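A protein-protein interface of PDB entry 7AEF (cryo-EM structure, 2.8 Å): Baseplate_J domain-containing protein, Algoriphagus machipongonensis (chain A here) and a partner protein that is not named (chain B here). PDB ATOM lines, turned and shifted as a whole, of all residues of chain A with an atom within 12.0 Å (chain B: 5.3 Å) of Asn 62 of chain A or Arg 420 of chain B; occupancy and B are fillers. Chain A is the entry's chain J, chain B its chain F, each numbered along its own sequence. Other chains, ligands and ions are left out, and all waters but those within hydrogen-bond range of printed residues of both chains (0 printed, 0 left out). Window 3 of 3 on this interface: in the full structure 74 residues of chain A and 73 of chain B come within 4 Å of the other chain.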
ATOM      1  N   ILE A  53      25.205  28.108 -18.743  1.00  0.00           N
ATOM      2  CA  ILE A  53      24.121  27.368 -18.111  1.00  0.00           C
ATOM      3  C   ILE A  53      24.710  26.157 -17.392  1.00  0.00           C
ATOM      4  O   ILE A  53      25.506  25.420 -17.977  1.00  0.00           O
ATOM      5  CB  ILE A  53      23.092  26.924 -19.169  1.00  0.00           C
ATOM      6  CG1 ILE A  53      22.539  28.121 -19.942  1.00  0.00           C
ATOM      7  CG2 ILE A  53      21.977  26.121 -18.560  1.00  0.00           C
ATOM      8  CD1 ILE A  53      21.803  29.137 -19.113  1.00  0.00           C
ATOM      9  N   HIS A  54      24.325  25.945 -16.134  1.00  0.00           N
ATOM     10  CA  HIS A  54      24.753  24.794 -15.338  1.00  0.00           C
ATOM     11  C   HIS A  54      24.160  23.508 -15.900  1.00  0.00           C
ATOM     12  O   HIS A  54      23.161  23.547 -16.598  1.00  0.00           O
ATOM     13  CB  HIS A  54      24.220  24.905 -13.921  1.00  0.00           C
ATOM     14  CG  HIS A  54      25.006  25.783 -13.004  1.00  0.00           C
ATOM     15  ND1 HIS A  54      24.401  26.622 -12.094  1.00  0.00           N
ATOM     16  CD2 HIS A  54      26.337  25.920 -12.810  1.00  0.00           C
ATOM     17  CE1 HIS A  54      25.322  27.254 -11.396  1.00  0.00           C
ATOM     18  NE2 HIS A  54      26.506  26.846 -11.811  1.00  0.00           N
ATOM     19  N   PHE A  55      24.773  22.359 -15.606  1.00  0.00           N
ATOM     20  CA  PHE A  55      24.205  21.069 -15.985  1.00  0.00           C
ATOM     21  C   PHE A  55      24.099  20.249 -14.724  1.00  0.00           C
ATOM     22  O   PHE A  55      25.038  20.203 -13.950  1.00  0.00           O
ATOM     23  CB  PHE A  55      25.032  20.295 -16.997  1.00  0.00           C
ATOM     24  CG  PHE A  55      24.430  18.980 -17.367  1.00  0.00           C
ATOM     25  CD1 PHE A  55      23.535  18.888 -18.403  1.00  0.00           C
ATOM     26  CD2 PHE A  55      24.744  17.825 -16.673  1.00  0.00           C
ATOM     27  CE1 PHE A  55      22.965  17.679 -18.730  1.00  0.00           C
ATOM     28  CE2 PHE A  55      24.174  16.630 -16.994  1.00  0.00           C
ATOM     29  CZ  PHE A  55      23.285  16.552 -18.025  1.00  0.00           C
ATOM     30  N   PHE A  56      22.988  19.558 -14.545  1.00  0.00           N
ATOM     31  CA  PHE A  56      22.743  18.785 -13.327  1.00  0.00           C
ATOM     32  C   PHE A  56      22.708  17.283 -13.574  1.00  0.00           C
ATOM     33  O   PHE A  56      21.717  16.782 -14.121  1.00  0.00           O
ATOM     34  CB  PHE A  56      21.427  19.212 -12.698  1.00  0.00           C
ATOM     35  CG  PHE A  56      21.445  20.578 -12.172  1.00  0.00           C
ATOM     36  CD1 PHE A  56      21.149  21.653 -12.975  1.00  0.00           C
ATOM     37  CD2 PHE A  56      21.756  20.788 -10.863  1.00  0.00           C
ATOM     38  CE1 PHE A  56      21.176  22.917 -12.471  1.00  0.00           C
ATOM     39  CE2 PHE A  56      21.780  22.046 -10.351  1.00  0.00           C
ATOM     40  CZ  PHE A  56      21.496  23.112 -11.151  1.00  0.00           C
ATOM     41  N   PRO A  57      23.737  16.544 -13.149  1.00  0.00           N
ATOM     42  CA  PRO A  57      23.792  15.082 -13.301  1.00  0.00           C
ATOM     43  C   PRO A  57      22.682  14.371 -12.553  1.00  0.00           C
ATOM     44  O   PRO A  57      22.283  14.789 -11.469  1.00  0.00           O
ATOM     45  CB  PRO A  57      25.147  14.733 -12.682  1.00  0.00           C
ATOM     46  CG  PRO A  57      25.917  15.974 -12.760  1.00  0.00           C
ATOM     47  CD  PRO A  57      24.966  17.085 -12.580  1.00  0.00           C
ATOM     48  N   SER A  58      22.250  13.228 -13.099  1.00  0.00           N
ATOM     49  CA  SER A  58      21.094  12.536 -12.542  1.00  0.00           C
ATOM     50  C   SER A  58      21.433  11.834 -11.221  1.00  0.00           C
ATOM     51  O   SER A  58      20.526  11.347 -10.544  1.00  0.00           O
ATOM     52  CB  SER A  58      20.587  11.406 -13.422  1.00  0.00           C
ATOM     53  OG  SER A  58      21.643  10.605 -13.887  1.00  0.00           O
ATOM     54  N   ASP A  59      22.706  11.715 -10.855  1.00  0.00           N
ATOM     55  CA  ASP A  59      23.077  11.041  -9.617  1.00  0.00           C
ATOM     56  C   ASP A  59      23.394  11.999  -8.469  1.00  0.00           C
ATOM     57  O   ASP A  59      23.849  11.550  -7.413  1.00  0.00           O
ATOM     58  CB  ASP A  59      24.260  10.119  -9.875  1.00  0.00           C
ATOM     59  CG  ASP A  59      25.403  10.839 -10.513  1.00  0.00           C
ATOM     60  OD1 ASP A  59      25.217  12.003 -10.888  1.00  0.00           O
ATOM     61  OD2 ASP A  59      26.491  10.267 -10.629  1.00  0.00           O
ATOM     62  N   LEU A  60      23.162  13.293  -8.630  1.00  0.00           N
ATOM     63  CA  LEU A  60      23.405  14.233  -7.549  1.00  0.00           C
ATOM     64  C   LEU A  60      22.090  14.859  -7.115  1.00  0.00           C
ATOM     65  O   LEU A  60      21.175  15.029  -7.916  1.00  0.00           O
ATOM     66  CB  LEU A  60      24.392  15.320  -7.973  1.00  0.00           C
ATOM     67  CG  LEU A  60      25.766  14.864  -8.474  1.00  0.00           C
ATOM     68  CD1 LEU A  60      26.567  16.066  -8.940  1.00  0.00           C
ATOM     69  CD2 LEU A  60      26.519  14.129  -7.392  1.00  0.00           C
ATOM     70  N   ALA A  61      22.001  15.245  -5.847  1.00  0.00           N
ATOM     71  CA  ALA A  61      20.770  15.844  -5.332  1.00  0.00           C
ATOM     72  C   ALA A  61      20.669  17.305  -5.735  1.00  0.00           C
ATOM     73  O   ALA A  61      20.772  18.205  -4.895  1.00  0.00           O
ATOM     74  CB  ALA A  61      20.713  15.730  -3.822  1.00  0.00           C
ATOM     75  N   ASN A  62      20.436  17.517  -7.024  1.00  0.00           N
ATOM     76  CA  ASN A  62      20.335  18.851  -7.568  1.00  0.00           C
ATOM     77  C   ASN A  62      21.609  19.659  -7.336  1.00  0.00           C
ATOM     78  O   ASN A  62      21.541  20.820  -6.965  1.00  0.00           O
ATOM     79  CB  ASN A  62      19.122  19.580  -6.986  1.00  0.00           C
ATOM     80  CG  ASN A  62      17.871  19.312  -7.751  1.00  0.00           C
ATOM     81  OD1 ASN A  62      17.926  18.933  -8.914  1.00  0.00           O
ATOM     82  ND2 ASN A  62      16.730  19.523  -7.119  1.00  0.00           N
ATOM     83  N   GLU A  63      22.764  19.048  -7.507  1.00  0.00           N
ATOM     84  CA  GLU A  63      24.003  19.797  -7.402  1.00  0.00           C
ATOM     85  C   GLU A  63      24.505  19.973  -8.819  1.00  0.00           C
ATOM     86  O   GLU A  63      24.373  19.050  -9.621  1.00  0.00           O
ATOM     87  CB  GLU A  63      25.001  18.966  -6.605  1.00  0.00           C
ATOM     88  CG  GLU A  63      24.702  18.833  -5.144  1.00  0.00           C
ATOM     89  CD  GLU A  63      25.678  17.911  -4.469  1.00  0.00           C
ATOM     90  OE1 GLU A  63      26.647  17.505  -5.121  1.00  0.00           O
ATOM     91  OE2 GLU A  63      25.545  17.672  -3.261  1.00  0.00           O
ATOM     92  N   PRO A  64      25.031  21.133  -9.172  1.00  0.00           N
ATOM     93  CA  PRO A  64      25.552  21.360 -10.525  1.00  0.00           C
ATOM     94  C   PRO A  64      26.912  20.709 -10.706  1.00  0.00           C
ATOM     95  O   PRO A  64      27.678  20.569  -9.753  1.00  0.00           O
ATOM     96  CB  PRO A  64      25.673  22.883 -10.580  1.00  0.00           C
ATOM     97  CG  PRO A  64      25.911  23.269  -9.142  1.00  0.00           C
ATOM     98  CD  PRO A  64      25.135  22.313  -8.312  1.00  0.00           C
ATOM     99  N   LEU A  65      27.213  20.302 -11.948  1.00  0.00           N
ATOM    100  CA  LEU A  65      28.548  19.780 -12.268  1.00  0.00           C
ATOM    101  C   LEU A  65      28.863  20.006 -13.752  1.00  0.00           C
ATOM    102  O   LEU A  65      28.698  19.105 -14.572  1.00  0.00           O
ATOM    103  CB  LEU A  65      28.620  18.300 -11.930  1.00  0.00           C
ATOM    104  CG  LEU A  65      29.966  17.587 -12.061  1.00  0.00           C
ATOM    105  CD1 LEU A  65      30.959  18.173 -11.094  1.00  0.00           C
ATOM    106  CD2 LEU A  65      29.773  16.114 -11.827  1.00  0.00           C
ATOM    107  N   GLY A  66      29.408  21.162 -14.082  1.00  0.00           N
ATOM    108  CA  GLY A  66      29.705  21.439 -15.482  1.00  0.00           C
ATOM    109  C   GLY A  66      28.576  22.154 -16.200  1.00  0.00           C
ATOM    110  O   GLY A  66      27.708  22.769 -15.578  1.00  0.00           O
ATOM    111  N   ASP A  67      28.579  22.055 -17.527  1.00  0.00           N
ATOM    112  CA  ASP A  67      27.687  22.840 -18.382  1.00  0.00           C
ATOM    113  C   ASP A  67      27.140  21.960 -19.513  1.00  0.00           C
ATOM    114  O   ASP A  67      27.241  20.733 -19.485  1.00  0.00           O
ATOM    115  CB  ASP A  67      28.424  24.087 -18.889  1.00  0.00           C
ATOM    116  CG  ASP A  67      29.644  23.753 -19.712  1.00  0.00           C
ATOM    117  OD1 ASP A  67      29.776  22.635 -20.193  1.00  0.00           O
ATOM    118  OD2 ASP A  67      30.533  24.596 -19.870  1.00  0.00           O
ATOM    119  N   TRP A  68      26.653  22.604 -20.572  1.00  0.00           N
ATOM    120  CA  TRP A  68      26.034  21.940 -21.710  1.00  0.00           C
ATOM    121  C   TRP A  68      26.932  21.904 -22.932  1.00  0.00           C
ATOM    122  O   TRP A  68      26.454  21.649 -24.042  1.00  0.00           O
ATOM    123  CB  TRP A  68      24.732  22.648 -22.033  1.00  0.00           C
ATOM    124  CG  TRP A  68      23.720  22.434 -21.005  1.00  0.00           C
ATOM    125  CD1 TRP A  68      23.630  23.035 -19.795  1.00  0.00           C
ATOM    126  CD2 TRP A  68      22.626  21.552 -21.097  1.00  0.00           C
ATOM    127  NE1 TRP A  68      22.545  22.573 -19.119  1.00  0.00           N
ATOM    128  CE2 TRP A  68      21.908  21.659 -19.908  1.00  0.00           C
ATOM    129  CE3 TRP A  68      22.174  20.678 -22.079  1.00  0.00           C
ATOM    130  CZ2 TRP A  68      20.778  20.928 -19.673  1.00  0.00           C
ATOM    131  CZ3 TRP A  68      21.054  19.961 -21.845  1.00  0.00           C
ATOM    132  CH2 TRP A  68      20.365  20.081 -20.660  1.00  0.00           C
ATOM    133  N   PHE A  71      26.961  19.138 -25.801  1.00  0.00           N
ATOM    134  CA  PHE A  71      25.797  18.850 -26.606  1.00  0.00           C
ATOM    135  C   PHE A  71      25.842  19.525 -27.969  1.00  0.00           C
ATOM    136  O   PHE A  71      25.031  19.187 -28.833  1.00  0.00           O
ATOM    137  CB  PHE A  71      24.550  19.241 -25.819  1.00  0.00           C
ATOM    138  CG  PHE A  71      24.290  18.350 -24.632  1.00  0.00           C
ATOM    139  CD1 PHE A  71      24.835  18.637 -23.398  1.00  0.00           C
ATOM    140  CD2 PHE A  71      23.509  17.219 -24.757  1.00  0.00           C
ATOM    141  CE1 PHE A  71      24.605  17.821 -22.319  1.00  0.00           C
ATOM    142  CE2 PHE A  71      23.274  16.407 -23.675  1.00  0.00           C
ATOM    143  CZ  PHE A  71      23.827  16.708 -22.461  1.00  0.00           C
ATOM    144  N   ALA B 416      11.978  13.836  -9.910  1.00  0.00           N
ATOM    145  CA  ALA B 416      12.156  15.281  -9.755  1.00  0.00           C
ATOM    146  C   ALA B 416      13.402  15.787 -10.476  1.00  0.00           C
ATOM    147  O   ALA B 416      13.390  16.863 -11.086  1.00  0.00           O
ATOM    148  CB  ALA B 416      12.243  15.628  -8.282  1.00  0.00           C
ATOM    149  N   VAL B 417      14.480  15.000 -10.440  1.00  0.00           N
ATOM    150  CA  VAL B 417      15.719  15.373 -11.117  1.00  0.00           C
ATOM    151  C   VAL B 417      15.522  15.430 -12.609  1.00  0.00           C
ATOM    152  O   VAL B 417      16.008  16.349 -13.280  1.00  0.00           O
ATOM    153  CB  VAL B 417      16.846  14.391 -10.789  1.00  0.00           C
ATOM    154  CG1 VAL B 417      18.064  14.663 -11.672  1.00  0.00           C
ATOM    155  CG2 VAL B 417      17.215  14.525  -9.352  1.00  0.00           C
ATOM    156  N   LEU B 418      14.842  14.427 -13.152  1.00  0.00           N
ATOM    157  CA  LEU B 418      14.603  14.388 -14.579  1.00  0.00           C
ATOM    158  C   LEU B 418      13.776  15.578 -15.029  1.00  0.00           C
ATOM    159  O   LEU B 418      13.965  16.070 -16.143  1.00  0.00           O
ATOM    160  CB  LEU B 418      13.909  13.085 -14.948  1.00  0.00           C
ATOM    161  CG  LEU B 418      14.730  11.796 -14.770  1.00  0.00           C
ATOM    162  CD1 LEU B 418      13.837  10.609 -15.012  1.00  0.00           C
ATOM    163  CD2 LEU B 418      15.914  11.759 -15.706  1.00  0.00           C
ATOM    164  N   ALA B 419      12.855  16.045 -14.187  1.00  0.00           N
ATOM    165  CA  ALA B 419      12.095  17.233 -14.544  1.00  0.00           C
ATOM    166  C   ALA B 419      13.009  18.433 -14.703  1.00  0.00           C
ATOM    167  O   ALA B 419      12.844  19.219 -15.640  1.00  0.00           O
ATOM    168  CB  ALA B 419      11.036  17.518 -13.500  1.00  0.00           C
ATOM    169  N   ARG B 420      13.999  18.558 -13.832  1.00  0.00           N
ATOM    170  CA  ARG B 420      14.944  19.646 -13.952  1.00  0.00           C
ATOM    171  C   ARG B 420      15.720  19.548 -15.249  1.00  0.00           C
ATOM    172  O   ARG B 420      15.953  20.561 -15.880  1.00  0.00           O
ATOM    173  CB  ARG B 420      15.888  19.664 -12.765  1.00  0.00           C
ATOM    174  CG  ARG B 420      16.463  21.028 -12.493  1.00  0.00           C
ATOM    175  CD  ARG B 420      17.050  21.098 -11.114  1.00  0.00           C
ATOM    176  NE  ARG B 420      16.102  21.656 -10.172  1.00  0.00           N
ATOM    177  CZ  ARG B 420      16.423  22.092  -8.968  1.00  0.00           C
ATOM    178  NH1 ARG B 420      15.495  22.590  -8.174  1.00  0.00           N
ATOM    179  NH2 ARG B 420      17.678  22.038  -8.559  1.00  0.00           N
ATOM    180  N   GLN B 421      16.104  18.342 -15.668  1.00  0.00           N
ATOM    181  CA  GLN B 421      16.834  18.178 -16.922  1.00  0.00           C
ATOM    182  C   GLN B 421      16.014  18.666 -18.099  1.00  0.00           C
ATOM    183  O   GLN B 421      16.542  19.329 -19.000  1.00  0.00           O
ATOM    184  CB  GLN B 421      17.208  16.723 -17.155  1.00  0.00           C
ATOM    185  CG  GLN B 421      18.233  16.170 -16.232  1.00  0.00           C
ATOM    186  CD  GLN B 421      18.514  14.740 -16.543  1.00  0.00           C
ATOM    187  OE1 GLN B 421      17.855  14.151 -17.390  1.00  0.00           O
ATOM    188  NE2 GLN B 421      19.489  14.168 -15.874  1.00  0.00           N
ATOM    189  N   LEU B 422      14.711  18.378 -18.086  1.00  0.00           N
ATOM    190  CA  LEU B 422      13.849  18.834 -19.167  1.00  0.00           C
ATOM    191  C   LEU B 422      13.738  20.347 -19.189  1.00  0.00           C
ATOM    192  O   LEU B 422      13.772  20.932 -20.274  1.00  0.00           O
ATOM    193  CB  LEU B 422      12.455  18.208 -19.082  1.00  0.00           C
ATOM    194  CG  LEU B 422      11.449  18.613 -20.194  1.00  0.00           C
ATOM    195  CD1 LEU B 422      11.978  18.274 -21.580  1.00  0.00           C
ATOM    196  CD2 LEU B 422      10.115  17.931 -19.967  1.00  0.00           C
ATOM    197  N   LYS B 423      13.618  20.999 -18.023  1.00  0.00           N
ATOM    198  CA  LYS B 423      13.533  22.460 -18.018  1.00  0.00           C
ATOM    199  C   LYS B 423      14.742  23.072 -18.697  1.00  0.00           C
ATOM    200  O   LYS B 423      14.600  23.995 -19.506  1.00  0.00           O
ATOM    201  CB  LYS B 423      13.457  23.011 -16.605  1.00  0.00           C
ATOM    202  CG  LYS B 423      12.192  22.727 -15.905  1.00  0.00           C
ATOM    203  CD  LYS B 423      12.190  23.301 -14.523  1.00  0.00           C
ATOM    204  CE  LYS B 423      10.931  22.905 -13.810  1.00  0.00           C
ATOM    205  NZ  LYS B 423      10.870  23.467 -12.455  1.00  0.00           N
ATOM    206  N   GLY B 424      15.917  22.509 -18.417  1.00  0.00           N
ATOM    207  CA  GLY B 424      17.140  22.971 -19.035  1.00  0.00           C
ATOM    208  C   GLY B 424      17.068  22.900 -20.540  1.00  0.00           C
ATOM    209  O   GLY B 424      17.320  23.885 -21.228  1.00  0.00           O
ATOM    210  N   ASP B 467      12.574  27.853 -11.321  1.00  0.00           N
ATOM    211  CA  ASP B 467      13.902  27.811 -10.731  1.00  0.00           C
ATOM    212  C   ASP B 467      15.003  28.492 -11.507  1.00  0.00           C
ATOM    213  O   ASP B 467      16.159  28.250 -11.173  1.00  0.00           O
ATOM    214  CB  ASP B 467      14.315  26.397 -10.371  1.00  0.00           C
ATOM    215  CG  ASP B 467      13.559  25.912  -9.175  1.00  0.00           C
ATOM    216  OD1 ASP B 467      12.995  26.730  -8.430  1.00  0.00           O
ATOM    217  OD2 ASP B 467      13.591  24.699  -8.930  1.00  0.00           O
ATOM    218  N   GLU B 470      18.492  28.743 -10.278  1.00  0.00           N
ATOM    219  CA  GLU B 470      19.366  27.594 -10.136  1.00  0.00           C
ATOM    220  C   GLU B 470      19.835  27.072 -11.479  1.00  0.00           C
ATOM    221  O   GLU B 470      20.945  26.542 -11.581  1.00  0.00           O
ATOM    222  CB  GLU B 470      18.655  26.482  -9.371  1.00  0.00           C
ATOM    223  CG  GLU B 470      18.285  26.855  -7.962  1.00  0.00           C
ATOM    224  CD  GLU B 470      17.666  25.719  -7.224  1.00  0.00           C
ATOM    225  OE1 GLU B 470      17.507  24.660  -7.816  1.00  0.00           O
ATOM    226  OE2 GLU B 470      17.342  25.879  -6.053  1.00  0.00           O
ATOM    227  N   LEU B 471      19.006  27.227 -12.508  1.00  0.00           N
ATOM    228  CA  LEU B 471      19.335  26.744 -13.844  1.00  0.00           C
ATOM    229  C   LEU B 471      20.516  27.504 -14.448  1.00  0.00           C
ATOM    230  O   LEU B 471      21.321  26.924 -15.183  1.00  0.00           O
ATOM    231  CB  LEU B 471      18.093  26.852 -14.744  1.00  0.00           C
ATOM    232  CG  LEU B 471      16.876  25.939 -14.412  1.00  0.00           C
ATOM    233  CD1 LEU B 471      15.658  26.343 -15.227  1.00  0.00           C
ATOM    234  CD2 LEU B 471      17.185  24.494 -14.702  1.00  0.00           C
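Of the printed residues of chain B, Ile 53 of chain A touches Leu 471.
Of the printed residues of chain B, His 54 of chain A touches Glu 470 and Leu 471.
Of the printed residues of chain B, Phe 56 of chain A touches Gln 421 (3.9 Å) and Glu 470 (3.5 Å).
Of the printed residues of chain B, Ser 58 of chain A touches Val 417 and Gln 421.
Of the printed residues of chain B, Asn 62 of chain A touches Arg 420.
No residue of chain A comes within 4 Å of Ala 416 of chain B.
Val 417 of chain B touches just one residue of chain A: Ser 58.
No residue of chain A comes within 4 Å of Ala 419 of chain B.
Of chain A, only Asn 62 comes within 4 Å of Arg 420 of chain B.
Of the printed residues of chain A, Gln 421 of chain B touches Phe 56 and Ser 58.
Leu 422 of chain B touches none of the printed residues of chain A.
No residue of chain A comes within 4 Å of Lys 423 of chain B.
No residue of chain A comes within 4 Å of Gly 424 of chain B.
No residue of chain A comes within 4 Å of Asp 467 of chain B.
Glu 470 of chain B touches two residues of chain A.
The nearest residue of chain B that does not touch Asn 62 of chain A is Val 417 of chain B (4.5 Å).
The nearest residue of chain A that does not touch Arg 420 of chain B is Phe 56 of chain A (4.5 Å).
Among the printed residues, pairs that only touch across the chains: Phe 56 of chain A with Glu 470 of chain B (3.5 Å), Ile 53 of chain A with Leu 471 of chain B (3.5 Å), Ser 58 of chain A with Val 417 of chain B (3.8 Å), Ser 58 of chain A with Gln 421 of chain B (3.9 Å) and Phe 56 of chain A with Gln 421 of chain B (3.9 Å).
ND2 of Asn 62 of chain A sits close to NH2 of Arg 420 of chain B (3.0 Å).
O of Glu 470 of chain B sits at hydrogen-bond distance from ND1 of His 54 of chain A, at 3.5 Å.
The backbone carbonyl oxygen of Leu 471 of chain B sits at hydrogen-bond distance from the backbone NH of His 54 of chain A, at 3.3 Å.
Hydrophobic or aromatic side chains of chain B that line the printed part of chain A: Val 417.
Among the printed residues, no Asp or Glu carboxylate lies within 4 Å of a Lys or Arg side-chain nitrogen of the other chain.
The guanidinium group of Arg 420 of chain B lies within salt-bridge range of the side-chain carboxylate of Asp 467 of chain B (2.9 Å).
OE1 of Glu 470 of chain B is in salt-bridge range of NH2 of Arg 420 of chain B (2.7 Å).
O of His 54 of chain A lies within hydrogen-bond range of NE1 of Trp 68 of chain A (2.8 Å).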
